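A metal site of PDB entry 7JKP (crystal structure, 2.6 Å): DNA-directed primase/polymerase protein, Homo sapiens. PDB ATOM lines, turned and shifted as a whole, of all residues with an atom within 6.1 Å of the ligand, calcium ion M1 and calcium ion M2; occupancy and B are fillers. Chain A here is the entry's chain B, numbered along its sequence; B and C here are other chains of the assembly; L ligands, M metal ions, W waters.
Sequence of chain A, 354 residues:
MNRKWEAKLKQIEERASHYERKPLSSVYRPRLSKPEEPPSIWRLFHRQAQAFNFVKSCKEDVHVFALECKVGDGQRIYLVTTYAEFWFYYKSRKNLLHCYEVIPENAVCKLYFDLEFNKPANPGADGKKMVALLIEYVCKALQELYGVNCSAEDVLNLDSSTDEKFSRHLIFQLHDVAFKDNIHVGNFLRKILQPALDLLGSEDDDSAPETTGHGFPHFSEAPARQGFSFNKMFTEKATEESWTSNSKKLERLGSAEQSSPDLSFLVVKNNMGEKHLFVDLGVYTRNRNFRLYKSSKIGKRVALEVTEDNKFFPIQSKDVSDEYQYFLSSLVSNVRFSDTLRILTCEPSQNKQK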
ATOM      1  N   GLY A  74      36.874  -5.364  10.654  1.00  0.00           N
ATOM      2  CA  GLY A  74      36.338  -4.762   9.452  1.00  0.00           C
ATOM      3  C   GLY A  74      36.330  -3.239   9.463  1.00  0.00           C
ATOM      4  O   GLY A  74      35.286  -2.615   9.295  1.00  0.00           O
ATOM      5  N   ARG A  76      36.833   0.586   8.159  1.00  0.00           N
ATOM      6  CA  ARG A  76      36.332   1.170   6.923  1.00  0.00           C
ATOM      7  C   ARG A  76      36.830   2.607   6.768  1.00  0.00           C
ATOM      8  O   ARG A  76      36.685   3.407   7.695  1.00  0.00           O
ATOM      9  CB  ARG A  76      34.798   1.158   6.870  1.00  0.00           C
ATOM     10  CG  ARG A  76      34.205   0.257   5.807  1.00  0.00           C
ATOM     11  CD  ARG A  76      34.256  -1.215   6.212  1.00  0.00           C
ATOM     12  NE  ARG A  76      33.355  -2.035   5.402  1.00  0.00           N
ATOM     13  CZ  ARG A  76      33.267  -3.354   5.492  1.00  0.00           C
ATOM     14  NH1 ARG A  76      34.029  -4.021   6.349  1.00  0.00           N
ATOM     15  NH2 ARG A  76      32.418  -4.014   4.711  1.00  0.00           N
ATOM     16  N   TYR A 100      33.458  -1.668  -1.388  1.00  0.00           N
ATOM     17  CA  TYR A 100      32.037  -1.852  -1.165  1.00  0.00           C
ATOM     18  C   TYR A 100      31.276  -0.607  -1.604  1.00  0.00           C
ATOM     19  O   TYR A 100      31.811   0.503  -1.579  1.00  0.00           O
ATOM     20  CB  TYR A 100      31.725  -2.153   0.316  1.00  0.00           C
ATOM     21  CG  TYR A 100      32.222  -3.491   0.778  1.00  0.00           C
ATOM     22  CD1 TYR A 100      33.527  -3.666   1.192  1.00  0.00           C
ATOM     23  CD2 TYR A 100      31.369  -4.597   0.807  1.00  0.00           C
ATOM     24  CE1 TYR A 100      33.994  -4.897   1.618  1.00  0.00           C
ATOM     25  CE2 TYR A 100      31.820  -5.833   1.229  1.00  0.00           C
ATOM     26  CZ  TYR A 100      33.129  -5.977   1.637  1.00  0.00           C
ATOM     27  OH  TYR A 100      33.591  -7.205   2.054  1.00  0.00           O
ATOM     28  N   ASP A 114      21.035 -10.813  -1.219  1.00  0.00           N
ATOM     29  CA  ASP A 114      22.238 -11.490  -0.741  1.00  0.00           C
ATOM     30  C   ASP A 114      21.847 -12.941  -0.470  1.00  0.00           C
ATOM     31  O   ASP A 114      21.102 -13.225   0.472  1.00  0.00           O
ATOM     32  CB  ASP A 114      22.801 -10.825   0.513  1.00  0.00           C
ATOM     33  CG  ASP A 114      24.131 -11.428   0.937  1.00  0.00           C
ATOM     34  OD1 ASP A 114      24.791 -12.088   0.104  1.00  0.00           O
ATOM     35  OD2 ASP A 114      24.526 -11.249   2.109  1.00  0.00           O
ATOM     36  N   LEU A 115      22.348 -13.859  -1.294  1.00  0.00           N
ATOM     37  CA  LEU A 115      21.987 -15.264  -1.219  1.00  0.00           C
ATOM     38  C   LEU A 115      23.159 -16.082  -0.719  1.00  0.00           C
ATOM     39  O   LEU A 115      24.324 -15.765  -0.975  1.00  0.00           O
ATOM     40  CB  LEU A 115      21.542 -15.781  -2.595  1.00  0.00           C
ATOM     41  CG  LEU A 115      20.426 -14.988  -3.279  1.00  0.00           C
ATOM     42  CD1 LEU A 115      20.000 -15.691  -4.564  1.00  0.00           C
ATOM     43  CD2 LEU A 115      19.232 -14.779  -2.363  1.00  0.00           C
ATOM     44  N   GLU A 116      22.846 -17.160   0.004  1.00  0.00           N
ATOM     45  CA  GLU A 116      23.873 -18.018   0.577  1.00  0.00           C
ATOM     46  C   GLU A 116      23.268 -19.193   1.337  1.00  0.00           C
ATOM     47  O   GLU A 116      22.483 -19.002   2.265  1.00  0.00           O
ATOM     48  CB  GLU A 116      24.773 -17.203   1.512  1.00  0.00           C
ATOM     49  CG  GLU A 116      24.040 -16.298   2.492  1.00  0.00           C
ATOM     50  CD  GLU A 116      24.892 -15.122   2.917  1.00  0.00           C
ATOM     51  OE1 GLU A 116      25.077 -14.919   4.141  1.00  0.00           O
ATOM     52  OE2 GLU A 116      25.380 -14.400   2.024  1.00  0.00           O
ATOM     53  N   SER A 160      29.766 -15.867  -6.313  1.00  0.00           N
ATOM     54  CA  SER A 160      30.916 -15.836  -5.401  1.00  0.00           C
ATOM     55  C   SER A 160      30.953 -17.088  -4.541  1.00  0.00           C
ATOM     56  O   SER A 160      31.412 -17.040  -3.390  1.00  0.00           O
ATOM     57  CB  SER A 160      30.863 -14.586  -4.513  1.00  0.00           C
ATOM     58  OG  SER A 160      31.976 -14.552  -3.629  1.00  0.00           O
ATOM     59  N   LYS A 165      30.088 -22.593   0.268  1.00  0.00           N
ATOM     60  CA  LYS A 165      28.924 -21.734   0.187  1.00  0.00           C
ATOM     61  C   LYS A 165      28.336 -21.732  -1.220  1.00  0.00           C
ATOM     62  O   LYS A 165      28.978 -22.150  -2.185  1.00  0.00           O
ATOM     63  CB  LYS A 165      29.266 -20.289   0.591  1.00  0.00           C
ATOM     64  CG  LYS A 165      30.196 -20.165   1.783  1.00  0.00           C
ATOM     65  CD  LYS A 165      31.642 -20.014   1.345  1.00  0.00           C
ATOM     66  CE  LYS A 165      32.592 -19.979   2.527  1.00  0.00           C
ATOM     67  NZ  LYS A 165      34.022 -19.919   2.095  1.00  0.00           N
ATOM     68  N   SER A 167      27.166 -18.630  -2.620  1.00  0.00           N
ATOM     69  CA  SER A 167      26.990 -17.188  -2.479  1.00  0.00           C
ATOM     70  C   SER A 167      26.651 -16.565  -3.818  1.00  0.00           C
ATOM     71  O   SER A 167      27.412 -16.702  -4.789  1.00  0.00           O
ATOM     72  CB  SER A 167      28.246 -16.561  -1.895  1.00  0.00           C
ATOM     73  OG  SER A 167      28.092 -15.161  -1.719  1.00  0.00           O
ATOM     74  N   ARG A 168      25.520 -15.866  -3.878  1.00  0.00           N
ATOM     75  CA  ARG A 168      25.075 -15.185  -5.093  1.00  0.00           C
ATOM     76  C   ARG A 168      24.545 -13.803  -4.725  1.00  0.00           C
ATOM     77  O   ARG A 168      23.981 -13.610  -3.653  1.00  0.00           O
ATOM     78  CB  ARG A 168      23.987 -15.968  -5.835  1.00  0.00           C
ATOM     79  CG  ARG A 168      24.385 -17.369  -6.246  1.00  0.00           C
ATOM     80  CD  ARG A 168      25.428 -17.354  -7.337  1.00  0.00           C
ATOM     81  NE  ARG A 168      25.659 -18.688  -7.888  1.00  0.00           N
ATOM     82  CZ  ARG A 168      24.835 -19.307  -8.727  1.00  0.00           C
ATOM     83  NH1 ARG A 168      23.705 -18.724  -9.117  1.00  0.00           N
ATOM     84  NH2 ARG A 168      25.141 -20.519  -9.169  1.00  0.00           N
ATOM     85  N   HIS A 169      24.748 -12.858  -5.636  1.00  0.00           N
ATOM     86  CA  HIS A 169      24.198 -11.512  -5.521  1.00  0.00           C
ATOM     87  C   HIS A 169      23.363 -11.228  -6.754  1.00  0.00           C
ATOM     88  O   HIS A 169      23.904 -11.177  -7.864  1.00  0.00           O
ATOM     89  CB  HIS A 169      25.303 -10.461  -5.367  1.00  0.00           C
ATOM     90  CG  HIS A 169      25.842 -10.341  -3.973  1.00  0.00           C
ATOM     91  ND1 HIS A 169      26.477  -9.209  -3.522  1.00  0.00           N
ATOM     92  CD2 HIS A 169      25.850 -11.217  -2.941  1.00  0.00           C
ATOM     93  CE1 HIS A 169      26.849  -9.391  -2.264  1.00  0.00           C
ATOM     94  NE2 HIS A 169      26.477 -10.597  -1.890  1.00  0.00           N
ATOM     95  N   ASP A 280      19.016 -13.716   2.553  1.00  0.00           N
ATOM     96  CA  ASP A 280      19.486 -12.958   3.706  1.00  0.00           C
ATOM     97  C   ASP A 280      18.704 -11.658   3.819  1.00  0.00           C
ATOM     98  O   ASP A 280      18.770 -10.801   2.929  1.00  0.00           O
ATOM     99  CB  ASP A 280      20.988 -12.682   3.571  1.00  0.00           C
ATOM    100  CG  ASP A 280      21.559 -11.937   4.763  1.00  0.00           C
ATOM    101  OD1 ASP A 280      20.795 -11.561   5.673  1.00  0.00           O
ATOM    102  OD2 ASP A 280      22.798 -11.719   4.787  1.00  0.00           O
ATOM    103  N   VAL A 283      20.417  -7.360   4.959  1.00  0.00           N
ATOM    104  CA  VAL A 283      21.208  -6.453   4.139  1.00  0.00           C
ATOM    105  C   VAL A 283      20.389  -5.231   3.689  1.00  0.00           C
ATOM    106  O   VAL A 283      20.730  -4.600   2.694  1.00  0.00           O
ATOM    107  CB  VAL A 283      21.818  -7.177   2.925  1.00  0.00           C
ATOM    108  CG1 VAL A 283      22.738  -8.294   3.388  1.00  0.00           C
ATOM    109  CG2 VAL A 283      20.716  -7.715   2.014  1.00  0.00           C
ATOM    110  N   ARG A 288      23.737   0.689   4.188  1.00  0.00           N
ATOM    111  CA  ARG A 288      24.264  -0.666   4.036  1.00  0.00           C
ATOM    112  C   ARG A 288      25.421  -0.677   3.054  1.00  0.00           C
ATOM    113  O   ARG A 288      25.422   0.036   2.043  1.00  0.00           O
ATOM    114  CB  ARG A 288      23.152  -1.613   3.571  1.00  0.00           C
ATOM    115  CG  ARG A 288      23.623  -2.971   3.067  1.00  0.00           C
ATOM    116  CD  ARG A 288      24.323  -3.784   4.144  1.00  0.00           C
ATOM    117  NE  ARG A 288      23.444  -4.083   5.273  1.00  0.00           N
ATOM    118  CZ  ARG A 288      23.834  -4.743   6.359  1.00  0.00           C
ATOM    119  NH1 ARG A 288      25.077  -5.177   6.470  1.00  0.00           N
ATOM    120  NH2 ARG A 288      22.966  -4.973   7.330  1.00  0.00           N
ATOM    121  N   ASN A 289      26.420  -1.503   3.351  1.00  0.00           N
ATOM    122  CA  ASN A 289      27.512  -1.775   2.423  1.00  0.00           C
ATOM    123  C   ASN A 289      27.188  -3.028   1.615  1.00  0.00           C
ATOM    124  O   ASN A 289      26.529  -3.953   2.090  1.00  0.00           O
ATOM    125  CB  ASN A 289      28.825  -1.962   3.173  1.00  0.00           C
ATOM    126  CG  ASN A 289      29.280  -0.692   3.875  1.00  0.00           C
ATOM    127  OD1 ASN A 289      28.554   0.294   3.923  1.00  0.00           O
ATOM    128  ND2 ASN A 289      30.489  -0.717   4.410  1.00  0.00           N
ATOM    129  N   PHE A 290      27.675  -3.051   0.374  1.00  0.00           N
ATOM    130  CA  PHE A 290      27.414  -4.176  -0.522  1.00  0.00           C
ATOM    131  C   PHE A 290      28.643  -4.401  -1.390  1.00  0.00           C
ATOM    132  O   PHE A 290      29.119  -3.473  -2.050  1.00  0.00           O
ATOM    133  CB  PHE A 290      26.171  -3.911  -1.388  1.00  0.00           C
ATOM    134  CG  PHE A 290      25.427  -5.154  -1.781  1.00  0.00           C
ATOM    135  CD1 PHE A 290      24.922  -6.005  -0.823  1.00  0.00           C
ATOM    136  CD2 PHE A 290      25.228  -5.455  -3.116  1.00  0.00           C
ATOM    137  CE1 PHE A 290      24.230  -7.153  -1.182  1.00  0.00           C
ATOM    138  CE2 PHE A 290      24.531  -6.601  -3.484  1.00  0.00           C
ATOM    139  CZ  PHE A 290      24.034  -7.444  -2.516  1.00  0.00           C
ATOM    140  N   ARG A 291      29.135  -5.640  -1.379  1.00  0.00           N
ATOM    141  CA  ARG A 291      30.380  -5.954  -2.074  1.00  0.00           C
ATOM    142  C   ARG A 291      30.259  -5.651  -3.560  1.00  0.00           C
ATOM    143  O   ARG A 291      29.261  -5.980  -4.201  1.00  0.00           O
ATOM    144  CB  ARG A 291      30.742  -7.424  -1.844  1.00  0.00           C
ATOM    145  CG  ARG A 291      32.125  -7.802  -2.348  1.00  0.00           C
ATOM    146  CD  ARG A 291      32.830  -8.740  -1.376  1.00  0.00           C
ATOM    147  NE  ARG A 291      32.129 -10.015  -1.191  1.00  0.00           N
ATOM    148  CZ  ARG A 291      32.205 -11.048  -2.021  1.00  0.00           C
ATOM    149  NH1 ARG A 291      32.951 -10.997  -3.118  1.00  0.00           N
ATOM    150  NH2 ARG A 291      31.530 -12.163  -1.749  1.00  0.00           N
ATOM    151  N   LYS A 297      36.122 -10.355   0.153  1.00  0.00           N
ATOM    152  CA  LYS A 297      36.357  -9.933   1.525  1.00  0.00           C
ATOM    153  C   LYS A 297      37.822  -9.551   1.723  1.00  0.00           C
ATOM    154  O   LYS A 297      38.694  -9.854   0.895  1.00  0.00           O
ATOM    155  CB  LYS A 297      35.930 -11.029   2.494  1.00  0.00           C
ATOM    156  CG  LYS A 297      34.413 -11.166   2.650  1.00  0.00           C
ATOM    157  CD  LYS A 297      34.012 -12.586   3.038  1.00  0.00           C
ATOM    158  CE  LYS A 297      32.718 -12.630   3.855  1.00  0.00           C
ATOM    159  NZ  LYS A 297      31.551 -12.069   3.133  1.00  0.00           N
ATOM    160  N   LEU A 304      33.201 -11.431  -6.586  1.00  0.00           N
ATOM    161  CA  LEU A 304      31.920 -11.375  -7.284  1.00  0.00           C
ATOM    162  C   LEU A 304      32.156 -11.331  -8.797  1.00  0.00           C
ATOM    163  O   LEU A 304      32.806 -10.421  -9.305  1.00  0.00           O
ATOM    164  CB  LEU A 304      31.122 -10.155  -6.829  1.00  0.00           C
ATOM    165  CG  LEU A 304      30.411 -10.289  -5.486  1.00  0.00           C
ATOM    166  CD1 LEU A 304      29.908  -8.938  -5.014  1.00  0.00           C
ATOM    167  CD2 LEU A 304      29.269 -11.286  -5.561  1.00  0.00           C
ATOM    168  P    DG B  13      26.842 -13.233  10.579  1.00  0.00           P
ATOM    169  OP1  DG B  13      26.039 -14.402  10.154  1.00  0.00           O
ATOM    170  OP2  DG B  13      28.324 -13.314  10.576  1.00  0.00           O
ATOM    171  O5'  DG B  13      26.434 -11.971   9.674  1.00  0.00           O
ATOM    172  C5'  DG B  13      25.075 -11.542   9.630  1.00  0.00           C
ATOM    173  C4'  DG B  13      24.935 -10.267   8.827  1.00  0.00           C
ATOM    174  O4'  DG B  13      25.648  -9.195   9.487  1.00  0.00           O
ATOM    175  C3'  DG B  13      25.508 -10.326   7.419  1.00  0.00           C
ATOM    176  O3'  DG B  13      24.763  -9.474   6.558  1.00  0.00           O
ATOM    177  C2'  DG B  13      26.932  -9.816   7.615  1.00  0.00           C
ATOM    178  C1'  DG B  13      26.728  -8.754   8.687  1.00  0.00           C
ATOM    179  N9   DG B  13      27.886  -8.562   9.546  1.00  0.00           N
ATOM    180  C8   DG B  13      28.790  -9.519   9.935  1.00  0.00           C
ATOM    181  N7   DG B  13      29.732  -9.065  10.718  1.00  0.00           N
ATOM    182  C5   DG B  13      29.437  -7.712  10.848  1.00  0.00           C
ATOM    183  C6   DG B  13      30.107  -6.699  11.582  1.00  0.00           C
ATOM    184  O6   DG B  13      31.135  -6.804  12.264  1.00  0.00           O
ATOM    185  N1   DG B  13      29.474  -5.465  11.444  1.00  0.00           N
ATOM    186  C2   DG B  13      28.341  -5.238  10.708  1.00  0.00           C
ATOM    187  N2   DG B  13      27.879  -3.977  10.700  1.00  0.00           N
ATOM    188  N3   DG B  13      27.701  -6.183  10.023  1.00  0.00           N
ATOM    189  C4   DG B  13      28.306  -7.384  10.138  1.00  0.00           C
ATOM    190  P   8OG C   3      37.370   2.589  13.439  1.00  0.00           P
ATOM    191  OP1 8OG C   3      37.208   1.481  14.470  1.00  0.00           O
ATOM    192  OP2 8OG C   3      38.768   2.648  12.931  1.00  0.00           O
ATOM    193  O5' 8OG C   3      36.302   2.395  12.215  1.00  0.00           O
ATOM    194  C5' 8OG C   3      36.302   3.330  11.195  1.00  0.00           C
ATOM    195  C4' 8OG C   3      35.043   3.185  10.364  1.00  0.00           C
ATOM    196  O4' 8OG C   3      34.880   1.966  10.002  1.00  0.00           O
ATOM    197  C3' 8OG C   3      33.717   3.616  11.243  1.00  0.00           C
ATOM    198  O3' 8OG C   3      33.035   4.763  10.568  1.00  0.00           O
ATOM    199  C2' 8OG C   3      32.974   2.632  11.297  1.00  0.00           C
ATOM    200  C1' 8OG C   3      33.412   1.751  10.067  1.00  0.00           C
ATOM    201  N9  8OG C   3      33.122   0.450  10.249  1.00  0.00           N
ATOM    202  C8  8OG C   3      32.130  -0.370   9.484  1.00  0.00           C
ATOM    203  N7  8OG C   3      32.196  -1.773  10.060  1.00  0.00           N
ATOM    204  C5  8OG C   3      33.198  -1.737  11.102  1.00  0.00           C
ATOM    205  C6  8OG C   3      33.699  -2.858  12.011  1.00  0.00           C
ATOM    206  O6  8OG C   3      33.226  -3.988  11.916  1.00  0.00           O
ATOM    207  N1  8OG C   3      34.739  -2.574  12.998  1.00  0.00           N
ATOM    208  C2  8OG C   3      35.292  -1.217  13.103  1.00  0.00           C
ATOM    209  N2  8OG C   3      36.359  -0.923  14.114  1.00  0.00           N
ATOM    210  N3  8OG C   3      34.814  -0.147  12.215  1.00  0.00           N
ATOM    211  C4  8OG C   3      33.750  -0.432  11.205  1.00  0.00           C
ATOM    212  O8  8OG C   3      31.433  -0.007   8.640  1.00  0.00           O
ATOM    213  P    DC C   4      31.947   5.638  11.358  1.00  0.00           P
ATOM    214  OP1  DC C   4      31.857   6.955  10.691  1.00  0.00           O
ATOM    215  OP2  DC C   4      32.269   5.565  12.796  1.00  0.00           O
ATOM    216  O5'  DC C   4      30.575   4.845  11.119  1.00  0.00           O
ATOM    217  C5'  DC C   4      30.056   4.720   9.805  1.00  0.00           C
ATOM    218  C4'  DC C   4      28.963   3.666   9.736  1.00  0.00           C
ATOM    219  O4'  DC C   4      29.514   2.370  10.069  1.00  0.00           O
ATOM    220  C3'  DC C   4      27.801   3.868  10.714  1.00  0.00           C
ATOM    221  O3'  DC C   4      26.668   4.425  10.033  1.00  0.00           O
ATOM    222  C2'  DC C   4      27.514   2.466  11.280  1.00  0.00           C
ATOM    223  C1'  DC C   4      28.459   1.547  10.502  1.00  0.00           C
ATOM    224  N1   DC C   4      29.024   0.420  11.297  1.00  0.00           N
ATOM    225  C2   DC C   4      28.508  -0.868  11.147  1.00  0.00           C
ATOM    226  O2   DC C   4      27.576  -1.062  10.360  1.00  0.00           O
ATOM    227  N3   DC C   4      29.047  -1.884  11.870  1.00  0.00           N
ATOM    228  C4   DC C   4      30.046  -1.643  12.717  1.00  0.00           C
ATOM    229  N4   DC C   4      30.542  -2.674  13.411  1.00  0.00           N
ATOM    230  C5   DC C   4      30.596  -0.335  12.879  1.00  0.00           C
ATOM    231  C6   DC C   4      30.064   0.657  12.157  1.00  0.00           C
HETATM  232  P1  LIG L   1      29.613 -13.842   0.961  1.00  0.00           P
HETATM  233  O1  LIG L   1      30.461 -14.759   1.845  1.00  0.00           O
HETATM  234  O2  LIG L   1      28.129 -14.088   1.243  1.00  0.00           O
HETATM  235  O3  LIG L   1      29.887 -14.127  -0.453  1.00  0.00           O
HETATM  236  P2  LIG L   1      29.022 -11.037   0.926  1.00  0.00           P
HETATM  237  O4  LIG L   1      29.662 -10.216  -0.198  1.00  0.00           O
HETATM  238  O5  LIG L   1      27.684 -11.558   0.445  1.00  0.00           O
HETATM  239  O6  LIG L   1      29.976 -12.300   1.299  1.00  0.00           O
HETATM  240  P3  LIG L   1      27.983 -10.508   3.639  1.00  0.00           P
HETATM  241  O7  LIG L   1      28.871 -10.353   4.849  1.00  0.00           O
HETATM  242  O8  LIG L   1      27.507 -11.949   3.519  1.00  0.00           O
HETATM  243  O9  LIG L   1      28.836 -10.076   2.260  1.00  0.00           O
HETATM  244  O10 LIG L   1      26.668  -9.508   3.795  1.00  0.00           O
HETATM  245  C1  LIG L   1      26.355  -8.631   2.718  1.00  0.00           C
HETATM  246  C2  LIG L   1      26.879  -7.239   3.030  1.00  0.00           C
HETATM  247  O11 LIG L   1      26.933  -7.041   4.271  1.00  0.00           O
HETATM  248  C3  LIG L   1      28.474  -7.053   2.550  1.00  0.00           C
HETATM  249  O12 LIG L   1      28.561  -6.981   1.073  1.00  0.00           O
HETATM  250  C4  LIG L   1      28.809  -5.997   3.059  1.00  0.00           C
HETATM  251  C5  LIG L   1      27.973  -5.938   4.413  1.00  0.00           C
HETATM  252  N1  LIG L   1      28.753  -6.147   5.429  1.00  0.00           N
HETATM  253  C6  LIG L   1      29.251  -7.303   5.860  1.00  0.00           C
HETATM  254  N2  LIG L   1      30.007  -7.040   6.934  1.00  0.00           N
HETATM  255  C7  LIG L   1      29.973  -5.715   7.169  1.00  0.00           C
HETATM  256  C8  LIG L   1      30.567  -4.928   8.132  1.00  0.00           C
HETATM  257  N3  LIG L   1      31.419  -5.078   9.255  1.00  0.00           N
HETATM  258  N4  LIG L   1      30.353  -3.615   8.131  1.00  0.00           N
HETATM  259  C9  LIG L   1      29.579  -3.060   7.193  1.00  0.00           C
HETATM  260  N5  LIG L   1      28.995  -3.830   6.242  1.00  0.00           N
HETATM  261  C10 LIG L   1      29.203  -5.162   6.240  1.00  0.00           C
HETATM  262 CA    CA M   1      25.028 -12.492   4.083  1.00  0.00          CA
HETATM  263 CA    CA M   2      26.592 -12.462   1.711  1.00  0.00          CA
HETATM  264  O   HOH W   1      26.265 -13.997  -0.213  1.00  0.00           O
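Arg 76 touches the ligand.
Tyr 100 touches the ligand (CE2 to O12, 3.5 Å).
Ser 160 touches the ligand (OG to O3, 3.8 Å).
Val 283 touches the ligand.
O of Asn 289 touches C4 of the ligand (3.2 Å).
Phe 290 touches the ligand.
Hydrophobic or aromatic side chains that line the ligand: Tyr 100, His 169 and Val 283.
15 residues have an atom within 4 Å of the ligand: Arg 76, Tyr 100, Asp 114, Glu 116, Ser 160, Ser 167, His 169, Val 283, Arg 288, Asn 289, Phe 290, Arg 291, Lys 297, DG 13 of chain B and 8OG 3 of chain C.
The nearest printed residue that does not touch the ligand is DC 4 of chain C (4.2 Å).
OG of Ser 167 is in hydrogen-bond range of O3 of the ligand.
The side-chain amino group (NZ) of Lys 297 is in salt-bridge range of an oxygen (O1) of the ligand, at 3.2 Å.
O12 of the ligand is in hydrogen-bond range of N of Arg 291 (2.9 Å).
The guanidinium group of Arg 291 lies within salt-bridge range of an oxygen (O4) of the ligand (2.7 Å).
A ring nitrogen (NE2) of His 169 sits close to an oxygen (O5) of the ligand.
A nitrogen (N3) of the ligand lies within hydrogen-bond range of N1 of DG 13 of chain B, at 3.0 Å.
A nitrogen (N3) of the ligand is in hydrogen-bond range of O6 of 8OG 3 of chain C (3.4 Å).
NH1 of Arg 288 is in hydrogen-bond range of O11 of the ligand, at 3.4 Å.
The side-chain carboxylate of Asp 114 lies close to a ring nitrogen (NE2) of His 169 (3.0 Å).
The backbone carbonyl oxygen (O) of Ser 167 is in hydrogen-bond range of the backbone NH (N) of Ser 160 (2.9 Å).
The side-chain hydroxyl of Ser 160 is in hydrogen-bond range of the guanidinium group of Arg 291, at 3.1 Å.
N2 of DG 13 of chain B lies close to N3 of DC 4 of chain C (2.7 Å).
ND2 of Asn 289 lies close to NE of Arg 76 (3.3 Å).
O4' of 8OG 3 of chain C lies within hydrogen-bond range of N of Arg 76 (3.0 Å).
The guanidinium group (NH1) of Arg 76 sits at hydrogen-bond distance from the backbone carbonyl oxygen (O) of Gly 74.
Two residues have an atom within 4 Å of calcium ion M2: Asp 114 and Glu 116.
Along chain A the residues within 4 Å of calcium ion M2 span positions 114 to 116.
The nearest printed residue that does not touch calcium ion M2 is His 169 (4.1 Å).
Merely in contact with calcium ion M1: DG 13 of chain B (3.9 Å).
The nearest printed residue that does not touch calcium ion M1 is Val 283 (4.8 Å).
Calcium ion M1 is bound by OD2 of Asp 114.
Calcium ion M1 is bound by OE1 of Glu 116, at 2.4 Å.
OD2 of Asp 280 is bound to calcium ion M1, 2.5 Å away.
O8 of the ligand binds calcium ion M1 (2.6 Å).
OE2 of Glu 116 binds calcium ion M1, at 2.8 Å.
Calcium ion M1 has five donor atoms within binding distance.
Water W1 lies within hydrogen-bond range of OG of Ser 167 (2.6 Å) and O of Leu 115 (2.7 Å).
Calcium ion M2 is bound by O5 of the ligand, O8 of the ligand, O2 of the ligand, OE2 of Glu 116, OD2 of Asp 114, OD1 of Asp 114 and water W1.
Calcium ion M2 has seven donor atoms within binding distance.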
